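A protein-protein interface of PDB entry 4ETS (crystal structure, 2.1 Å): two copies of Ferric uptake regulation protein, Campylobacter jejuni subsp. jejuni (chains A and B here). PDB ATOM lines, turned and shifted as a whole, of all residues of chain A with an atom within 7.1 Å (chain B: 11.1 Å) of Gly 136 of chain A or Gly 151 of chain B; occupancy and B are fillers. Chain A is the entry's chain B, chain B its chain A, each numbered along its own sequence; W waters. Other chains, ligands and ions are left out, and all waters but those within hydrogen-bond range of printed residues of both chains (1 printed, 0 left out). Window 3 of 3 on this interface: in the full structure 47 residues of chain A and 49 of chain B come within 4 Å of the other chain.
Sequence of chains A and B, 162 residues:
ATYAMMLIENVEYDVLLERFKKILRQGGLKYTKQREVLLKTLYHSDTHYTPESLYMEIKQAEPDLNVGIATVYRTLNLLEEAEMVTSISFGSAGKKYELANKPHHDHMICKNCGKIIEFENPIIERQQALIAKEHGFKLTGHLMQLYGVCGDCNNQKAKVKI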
ATOM      1  N   LEU A 130       2.769 -22.726  35.843  1.00  0.00           N
ATOM      2  CA  LEU A 130       3.591 -22.375  37.012  1.00  0.00           C
ATOM      3  C   LEU A 130       5.095 -22.355  36.726  1.00  0.00           C
ATOM      4  O   LEU A 130       5.794 -21.445  37.158  1.00  0.00           O
ATOM      5  CB  LEU A 130       3.312 -23.397  38.108  1.00  0.00           C
ATOM      6  CG  LEU A 130       3.365 -23.087  39.610  1.00  0.00           C
ATOM      7  CD1 LEU A 130       3.545 -24.353  40.556  1.00  0.00           C
ATOM      8  CD2 LEU A 130       4.283 -21.910  40.041  1.00  0.00           C
ATOM      9  N   ILE A 131       5.623 -23.377  36.013  1.00  0.00           N
ATOM     10  CA  ILE A 131       6.998 -23.380  35.701  1.00  0.00           C
ATOM     11  C   ILE A 131       7.426 -22.127  34.857  1.00  0.00           C
ATOM     12  O   ILE A 131       8.471 -21.464  35.096  1.00  0.00           O
ATOM     13  CB  ILE A 131       7.308 -24.699  34.899  1.00  0.00           C
ATOM     14  CG1 ILE A 131       7.152 -25.922  35.802  1.00  0.00           C
ATOM     15  CG2 ILE A 131       8.669 -24.600  34.232  1.00  0.00           C
ATOM     16  CD1 ILE A 131       6.983 -27.185  34.938  1.00  0.00           C
ATOM     17  N   ALA A 132       6.617 -21.800  33.880  1.00  0.00           N
ATOM     18  CA  ALA A 132       6.893 -20.638  33.056  1.00  0.00           C
ATOM     19  C   ALA A 132       6.942 -19.400  34.002  1.00  0.00           C
ATOM     20  O   ALA A 132       7.958 -18.690  34.041  1.00  0.00           O
ATOM     21  CB  ALA A 132       5.783 -20.486  31.990  1.00  0.00           C
ATOM     22  N   LYS A 133       5.860 -19.184  34.767  1.00  0.00           N
ATOM     23  CA  LYS A 133       5.759 -18.043  35.743  1.00  0.00           C
ATOM     24  C   LYS A 133       6.955 -17.960  36.694  1.00  0.00           C
ATOM     25  O   LYS A 133       7.515 -16.878  36.902  1.00  0.00           O
ATOM     26  CB  LYS A 133       4.473 -18.163  36.580  1.00  0.00           C
ATOM     27  CG  LYS A 133       4.253 -17.024  37.646  1.00  0.00           C
ATOM     28  CD  LYS A 133       2.752 -16.897  38.002  1.00  0.00           C
ATOM     29  CE  LYS A 133       2.508 -15.723  38.967  1.00  0.00           C
ATOM     30  NZ  LYS A 133       1.557 -16.075  40.087  1.00  0.00           N
ATOM     31  N   GLU A 134       7.347 -19.087  37.283  1.00  0.00           N
ATOM     32  CA  GLU A 134       8.472 -19.103  38.225  1.00  0.00           C
ATOM     33  C   GLU A 134       9.759 -18.643  37.603  1.00  0.00           C
ATOM     34  O   GLU A 134      10.667 -18.259  38.329  1.00  0.00           O
ATOM     35  CB  GLU A 134       8.761 -20.511  38.821  1.00  0.00           C
ATOM     36  CG  GLU A 134       7.695 -21.037  39.740  1.00  0.00           C
ATOM     37  CD  GLU A 134       7.927 -22.516  40.122  1.00  0.00           C
ATOM     38  OE1 GLU A 134       7.444 -22.918  41.200  1.00  0.00           O
ATOM     39  OE2 GLU A 134       8.580 -23.291  39.366  1.00  0.00           O
ATOM     40  N   HIS A 135       9.911 -18.770  36.288  1.00  0.00           N
ATOM     41  CA  HIS A 135      11.188 -18.374  35.678  1.00  0.00           C
ATOM     42  C   HIS A 135      11.067 -17.112  34.870  1.00  0.00           C
ATOM     43  O   HIS A 135      11.945 -16.815  34.079  1.00  0.00           O
ATOM     44  CB  HIS A 135      11.701 -19.498  34.792  1.00  0.00           C
ATOM     45  CG  HIS A 135      12.080 -20.708  35.565  1.00  0.00           C
ATOM     46  ND1 HIS A 135      13.280 -20.805  36.239  1.00  0.00           N
ATOM     47  CD2 HIS A 135      11.373 -21.820  35.882  1.00  0.00           C
ATOM     48  CE1 HIS A 135      13.344 -21.979  36.834  1.00  0.00           C
ATOM     49  NE2 HIS A 135      12.198 -22.608  36.643  1.00  0.00           N
ATOM     50  N   GLY A 136       9.937 -16.419  35.043  1.00  0.00           N
ATOM     51  CA  GLY A 136       9.667 -15.133  34.382  1.00  0.00           C
ATOM     52  C   GLY A 136       9.240 -15.255  32.907  1.00  0.00           C
ATOM     53  O   GLY A 136       9.195 -14.237  32.190  1.00  0.00           O
ATOM     54  N   PHE A 137       8.955 -16.476  32.428  1.00  0.00           N
ATOM     55  CA  PHE A 137       8.618 -16.682  30.996  1.00  0.00           C
ATOM     56  C   PHE A 137       7.157 -16.543  30.788  1.00  0.00           C
ATOM     57  O   PHE A 137       6.346 -16.840  31.695  1.00  0.00           O
ATOM     58  CB  PHE A 137       8.914 -18.114  30.499  1.00  0.00           C
ATOM     59  CG  PHE A 137      10.328 -18.367  30.050  1.00  0.00           C
ATOM     60  CD1 PHE A 137      11.414 -18.191  30.930  1.00  0.00           C
ATOM     61  CD2 PHE A 137      10.575 -18.825  28.769  1.00  0.00           C
ATOM     62  CE1 PHE A 137      12.712 -18.434  30.512  1.00  0.00           C
ATOM     63  CE2 PHE A 137      11.867 -19.116  28.330  1.00  0.00           C
ATOM     64  CZ  PHE A 137      12.965 -18.904  29.190  1.00  0.00           C
ATOM     65  N   LYS A 138       6.825 -16.149  29.552  1.00  0.00           N
ATOM     66  CA  LYS A 138       5.478 -16.196  29.012  1.00  0.00           C
ATOM     67  C   LYS A 138       5.483 -17.437  28.141  1.00  0.00           C
ATOM     68  O   LYS A 138       6.335 -17.616  27.241  1.00  0.00           O
ATOM     69  CB  LYS A 138       5.241 -14.922  28.146  1.00  0.00           C
ATOM     70  CG  LYS A 138       3.883 -14.844  27.444  1.00  0.00           C
ATOM     71  CD  LYS A 138       3.736 -13.591  26.522  1.00  0.00           C
ATOM     72  CE  LYS A 138       5.008 -13.364  25.686  1.00  0.00           C
ATOM     73  NZ  LYS A 138       4.900 -12.145  24.809  1.00  0.00           N
ATOM     74  N   MET B 108      12.643 -25.752  28.905  1.00  0.00           N
ATOM     75  CA  MET B 108      11.865 -24.605  28.494  1.00  0.00           C
ATOM     76  C   MET B 108      12.765 -23.667  27.670  1.00  0.00           C
ATOM     77  O   MET B 108      13.862 -23.278  28.125  1.00  0.00           O
ATOM     78  CB  MET B 108      11.296 -23.906  29.714  1.00  0.00           C
ATOM     79  CG  MET B 108      10.527 -22.614  29.410  1.00  0.00           C
ATOM     80  SD  MET B 108       9.634 -21.949  30.850  1.00  0.00           S
ATOM     81  CE  MET B 108       7.976 -22.498  30.522  1.00  0.00           C
ATOM     82  N   ILE B 109      12.310 -23.288  26.468  1.00  0.00           N
ATOM     83  CA  ILE B 109      13.164 -22.582  25.496  1.00  0.00           C
ATOM     84  C   ILE B 109      12.606 -21.183  25.179  1.00  0.00           C
ATOM     85  O   ILE B 109      11.452 -21.071  24.814  1.00  0.00           O
ATOM     86  CB  ILE B 109      13.249 -23.436  24.173  1.00  0.00           C
ATOM     87  CG1 ILE B 109      13.881 -24.784  24.502  1.00  0.00           C
ATOM     88  CG2 ILE B 109      14.011 -22.696  23.065  1.00  0.00           C
ATOM     89  CD1 ILE B 109      13.722 -25.863  23.464  1.00  0.00           C
ATOM     90  N   CYS B 110      13.415 -20.123  25.317  1.00  0.00           N
ATOM     91  CA  CYS B 110      12.973 -18.792  24.929  1.00  0.00           C
ATOM     92  C   CYS B 110      13.057 -18.713  23.387  1.00  0.00           C
ATOM     93  O   CYS B 110      14.117 -18.914  22.867  1.00  0.00           O
ATOM     94  CB  CYS B 110      13.854 -17.644  25.495  1.00  0.00           C
ATOM     95  SG  CYS B 110      13.252 -16.085  24.829  1.00  0.00           S
ATOM     96  N   LYS B 111      11.943 -18.397  22.728  1.00  0.00           N
ATOM     97  CA  LYS B 111      11.820 -18.320  21.234  1.00  0.00           C
ATOM     98  C   LYS B 111      12.724 -17.185  20.661  1.00  0.00           C
ATOM     99  O   LYS B 111      13.126 -17.214  19.500  1.00  0.00           O
ATOM    100  CB  LYS B 111      10.343 -18.078  20.815  1.00  0.00           C
ATOM    101  CG  LYS B 111       9.463 -19.370  20.862  1.00  0.00           C
ATOM    102  CD  LYS B 111       7.948 -19.245  20.324  1.00  0.00           C
ATOM    103  CE  LYS B 111       7.044 -20.344  21.073  1.00  0.00           C
ATOM    104  NZ  LYS B 111       5.664 -20.991  20.564  1.00  0.00           N
ATOM    105  N   ASN B 112      13.063 -16.221  21.488  1.00  0.00           N
ATOM    106  CA  ASN B 112      13.895 -15.121  21.026  1.00  0.00           C
ATOM    107  C   ASN B 112      15.389 -15.325  21.231  1.00  0.00           C
ATOM    108  O   ASN B 112      16.129 -15.617  20.277  1.00  0.00           O
ATOM    109  CB  ASN B 112      13.435 -13.801  21.628  1.00  0.00           C
ATOM    110  CG  ASN B 112      14.096 -12.597  20.951  1.00  0.00           C
ATOM    111  OD1 ASN B 112      15.186 -12.717  20.357  1.00  0.00           O
ATOM    112  ND2 ASN B 112      13.448 -11.433  21.052  1.00  0.00           N
ATOM    113  N   CYS B 113      15.864 -15.176  22.452  1.00  0.00           N
ATOM    114  CA  CYS B 113      17.303 -15.257  22.674  1.00  0.00           C
ATOM    115  C   CYS B 113      17.840 -16.671  22.710  1.00  0.00           C
ATOM    116  O   CYS B 113      19.029 -16.836  22.795  1.00  0.00           O
ATOM    117  CB  CYS B 113      17.641 -14.585  24.006  1.00  0.00           C
ATOM    118  SG  CYS B 113      16.843 -15.366  25.513  1.00  0.00           S
ATOM    119  N   GLY B 114      16.975 -17.695  22.750  1.00  0.00           N
ATOM    120  CA  GLY B 114      17.447 -19.083  22.845  1.00  0.00           C
ATOM    121  C   GLY B 114      17.957 -19.517  24.217  1.00  0.00           C
ATOM    122  O   GLY B 114      18.597 -20.507  24.326  1.00  0.00           O
ATOM    123  N   LYS B 115      17.685 -18.780  25.267  1.00  0.00           N
ATOM    124  CA  LYS B 115      17.986 -19.250  26.630  1.00  0.00           C
ATOM    125  C   LYS B 115      17.154 -20.539  26.952  1.00  0.00           C
ATOM    126  O   LYS B 115      15.984 -20.635  26.559  1.00  0.00           O
ATOM    127  CB  LYS B 115      17.571 -18.140  27.590  1.00  0.00           C
ATOM    128  CG  LYS B 115      17.317 -18.582  28.988  1.00  0.00           C
ATOM    129  CD  LYS B 115      16.815 -17.438  29.818  1.00  0.00           C
ATOM    130  CE  LYS B 115      17.067 -17.707  31.302  1.00  0.00           C
ATOM    131  NZ  LYS B 115      16.172 -16.842  32.142  1.00  0.00           N
ATOM    132  N   ILE B 116      17.749 -21.483  27.686  1.00  0.00           N
ATOM    133  CA  ILE B 116      17.103 -22.743  27.938  1.00  0.00           C
ATOM    134  C   ILE B 116      17.106 -22.945  29.449  1.00  0.00           C
ATOM    135  O   ILE B 116      18.114 -22.702  30.111  1.00  0.00           O
ATOM    136  CB  ILE B 116      17.804 -23.919  27.311  1.00  0.00           C
ATOM    137  CG1 ILE B 116      18.029 -23.736  25.795  1.00  0.00           C
ATOM    138  CG2 ILE B 116      17.070 -25.257  27.629  1.00  0.00           C
ATOM    139  CD1 ILE B 116      16.960 -23.064  25.105  1.00  0.00           C
ATOM    140  N   ILE B 117      15.980 -23.398  29.985  1.00  0.00           N
ATOM    141  CA  ILE B 117      15.900 -23.723  31.392  1.00  0.00           C
ATOM    142  C   ILE B 117      15.662 -25.209  31.373  1.00  0.00           C
ATOM    143  O   ILE B 117      14.693 -25.694  30.726  1.00  0.00           O
ATOM    144  CB  ILE B 117      14.645 -23.058  32.070  1.00  0.00           C
ATOM    145  CG1 ILE B 117      14.691 -21.518  32.013  1.00  0.00           C
ATOM    146  CG2 ILE B 117      14.440 -23.569  33.604  1.00  0.00           C
ATOM    147  CD1 ILE B 117      15.931 -20.884  32.614  1.00  0.00           C
ATOM    148  N   LEU B 146       8.716 -26.807  26.648  1.00  0.00           N
ATOM    149  CA  LEU B 146       7.859 -25.640  26.773  1.00  0.00           C
ATOM    150  C   LEU B 146       8.542 -24.557  25.919  1.00  0.00           C
ATOM    151  O   LEU B 146       9.789 -24.439  25.880  1.00  0.00           O
ATOM    152  CB  LEU B 146       7.764 -25.205  28.245  1.00  0.00           C
ATOM    153  CG  LEU B 146       7.395 -26.322  29.271  1.00  0.00           C
ATOM    154  CD1 LEU B 146       7.204 -25.727  30.731  1.00  0.00           C
ATOM    155  CD2 LEU B 146       6.081 -26.965  28.852  1.00  0.00           C
ATOM    156  N   TYR B 147       7.735 -23.816  25.190  1.00  0.00           N
ATOM    157  CA  TYR B 147       8.285 -22.721  24.366  1.00  0.00           C
ATOM    158  C   TYR B 147       7.645 -21.443  24.809  1.00  0.00           C
ATOM    159  O   TYR B 147       6.457 -21.421  25.138  1.00  0.00           O
ATOM    160  CB  TYR B 147       7.982 -22.956  22.893  1.00  0.00           C
ATOM    161  CG  TYR B 147       8.296 -24.378  22.418  1.00  0.00           C
ATOM    162  CD1 TYR B 147       9.612 -24.794  22.244  1.00  0.00           C
ATOM    163  CD2 TYR B 147       7.262 -25.277  22.121  1.00  0.00           C
ATOM    164  CE1 TYR B 147       9.896 -26.162  21.821  1.00  0.00           C
ATOM    165  CE2 TYR B 147       7.524 -26.603  21.703  1.00  0.00           C
ATOM    166  CZ  TYR B 147       8.851 -27.007  21.549  1.00  0.00           C
ATOM    167  OH  TYR B 147       9.105 -28.282  21.131  1.00  0.00           O
ATOM    168  N   GLY B 148       8.438 -20.398  24.895  1.00  0.00           N
ATOM    169  CA  GLY B 148       7.919 -19.133  25.379  1.00  0.00           C
ATOM    170  C   GLY B 148       8.894 -18.007  25.139  1.00  0.00           C
ATOM    171  O   GLY B 148       9.797 -18.132  24.304  1.00  0.00           O
ATOM    172  N   VAL B 149       8.702 -16.894  25.843  1.00  0.00           N
ATOM    173  CA  VAL B 149       9.601 -15.765  25.695  1.00  0.00           C
ATOM    174  C   VAL B 149      10.021 -15.404  27.099  1.00  0.00           C
ATOM    175  O   VAL B 149       9.189 -15.249  27.985  1.00  0.00           O
ATOM    176  CB  VAL B 149       8.916 -14.544  24.965  1.00  0.00           C
ATOM    177  CG1 VAL B 149       9.820 -13.320  24.961  1.00  0.00           C
ATOM    178  CG2 VAL B 149       8.537 -14.896  23.465  1.00  0.00           C
ATOM    179  N   CYS B 150      11.324 -15.301  27.320  1.00  0.00           N
ATOM    180  CA  CYS B 150      11.796 -14.991  28.671  1.00  0.00           C
ATOM    181  C   CYS B 150      11.463 -13.551  29.063  1.00  0.00           C
ATOM    182  O   CYS B 150      10.966 -12.742  28.226  1.00  0.00           O
ATOM    183  CB  CYS B 150      13.299 -15.291  28.811  1.00  0.00           C
ATOM    184  SG  CYS B 150      14.353 -14.049  28.013  1.00  0.00           S
ATOM    185  N   GLY B 151      11.715 -13.260  30.348  1.00  0.00           N
ATOM    186  CA  GLY B 151      11.462 -11.953  30.953  1.00  0.00           C
ATOM    187  C   GLY B 151      12.251 -10.855  30.261  1.00  0.00           C
ATOM    188  O   GLY B 151      11.706  -9.780  29.959  1.00  0.00           O
ATOM    189  N   ASP B 152      13.509 -11.129  29.974  1.00  0.00           N
ATOM    190  CA  ASP B 152      14.332 -10.168  29.245  1.00  0.00           C
ATOM    191  C   ASP B 152      13.836  -9.907  27.804  1.00  0.00           C
ATOM    192  O   ASP B 152      13.911  -8.783  27.335  1.00  0.00           O
ATOM    193  CB  ASP B 152      15.782 -10.635  29.213  1.00  0.00           C
ATOM    194  CG  ASP B 152      16.375 -10.764  30.597  1.00  0.00           C
ATOM    195  OD1 ASP B 152      15.839 -10.151  31.542  1.00  0.00           O
ATOM    196  OD2 ASP B 152      17.394 -11.468  30.745  1.00  0.00           O
ATOM    197  N   CYS B 153      13.359 -10.933  27.101  1.00  0.00           N
ATOM    198  CA  CYS B 153      12.884 -10.717  25.729  1.00  0.00           C
ATOM    199  C   CYS B 153      11.408 -10.370  25.667  1.00  0.00           C
ATOM    200  O   CYS B 153      10.853 -10.324  24.561  1.00  0.00           O
ATOM    201  CB  CYS B 153      13.124 -11.946  24.851  1.00  0.00           C
ATOM    202  SG  CYS B 153      14.799 -12.431  24.706  1.00  0.00           S
ATOM    203  N   ASN B 154      10.760 -10.232  26.824  1.00  0.00           N
ATOM    204  CA  ASN B 154       9.356  -9.843  26.953  1.00  0.00           C
ATOM    205  C   ASN B 154       8.420 -10.570  27.912  1.00  0.00           C
ATOM    206  O   ASN B 154       7.193 -10.421  27.786  1.00  0.00           O
ATOM    207  CB  ASN B 154       8.677  -9.678  25.584  1.00  0.00           C
ATOM    208  CG  ASN B 154       8.699  -8.249  25.132  1.00  0.00           C
ATOM    209  OD1 ASN B 154       9.733  -7.595  25.297  1.00  0.00           O
ATOM    210  ND2 ASN B 154       7.559  -7.727  24.602  1.00  0.00           N
HETATM  211  O   HOH W   1      13.085 -14.841  32.379  1.00  0.00           O
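No position is printed for both chains.
Of the 13 pairs that touch across the chains among the printed residues, none has its exchanged pair printed and touching as well.
O of Lys 138 of chain A sits at hydrogen-bond distance from N of Val 149 of chain B (2.8 Å).
N of Gly 151 of chain B is in hydrogen-bond range of O of Gly 136 of chain A, at 3.3 Å.
Of the printed residues of chain B, Ile 131 of chain A touches Leu 146.
Of chain B, only Cys 150 (3.9 Å) and Gly 151 (3.3 Å) come within 4 Å of Gly 136 of chain A.
Printed residues of chain A within 4 Å of Leu 146 of chain B: Ile 131.
Of the printed residues of chain A, Val 149 of chain B touches Phe 137 (3.4 Å) and Lys 138 (2.8 Å).
Of the printed residues of chain A, Cys 150 of chain B touches Gly 136 (3.9 Å) and Phe 137 (3.6 Å).
Gly 151 of chain B touches just one residue of chain A: Gly 136.
The nearest residue of chain B that does not touch Gly 136 of chain A is Val 149 of chain B (4.3 Å).
The nearest printed residue of chain B that does not touch Phe 137 of chain A is Gly 148 of chain B (4.1 Å).
Printed residues of chain B that touch a printed residue of chain A: Met 108, Ile 109, Cys 110, Ile 117, Leu 146, Gly 148, Val 149, Cys 150 and Gly 151.
Hydrophobic or aromatic side chains of chain B that line the printed part of chain A: Met 108, Ile 117 and Leu 146.
Hydrophobic or aromatic side chains of chain A within 4 Å of the printed part of chain B: Ile 131, Ala 132, His 135 and Phe 137.
Among the printed residues, 13 pairs touch across the chains.
Among the printed residues, no Asp or Glu carboxylate lies within 4 Å of a Lys or Arg side-chain nitrogen of the other chain.
The backbone NH (N) of Asp 152 of chain B lies close to the side-chain sulfur (SG) of Cys 150 of chain B, 3.6 Å away.
O of Ala 132 of chain A sits at hydrogen-bond distance from N of Phe 137 of chain A, 2.9 Å away.
O of Leu 146 of chain B sits at hydrogen-bond distance from N of Ile 109 of chain B.
O of Lys 115 of chain B lies within hydrogen-bond range of N of Cys 110 of chain B, 2.9 Å away.
The backbone carbonyl oxygen of Ile 109 of chain B sits at hydrogen-bond distance from the backbone NH of Gly 148 of chain B.
The backbone NH (N) of Lys 111 of chain B lies within hydrogen-bond range of the backbone carbonyl oxygen (O) of Gly 148 of chain B, 2.7 Å away.
Leu 146 of chain B touches Ile 131 of chain A (CD1 to CG2, 3.96 Å).
Met 108 of chain B touches Ala 132 of chain A (CE to CB, 3.3 Å).
His 135 of chain A touches Ile 117 of chain B.
O of Gly 136 of chain A touches C of Cys 150 of chain B, at 3.9 Å.
Phe 137 of chain A touches Met 108 of chain B (CG to SD, 3.7 Å).
CE2 of Phe 137 of chain A touches C of Ile 109 of chain B (3.8 Å).
Cys 110 of chain B touches Phe 137 of chain A (N to CE2, 3.5 Å).
Phe 137 of chain A touches Ile 117 of chain B.
CE1 of Phe 137 of chain A touches CB of Cys 150 of chain B (3.6 Å).
O of Lys 138 of chain A touches CA of Gly 148 of chain B (2.9 Å).
Water W1 lies within hydrogen-bond range of O of His 135 of chain A (2.8 Å) and N of Gly 151 of chain B (2.9 Å).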
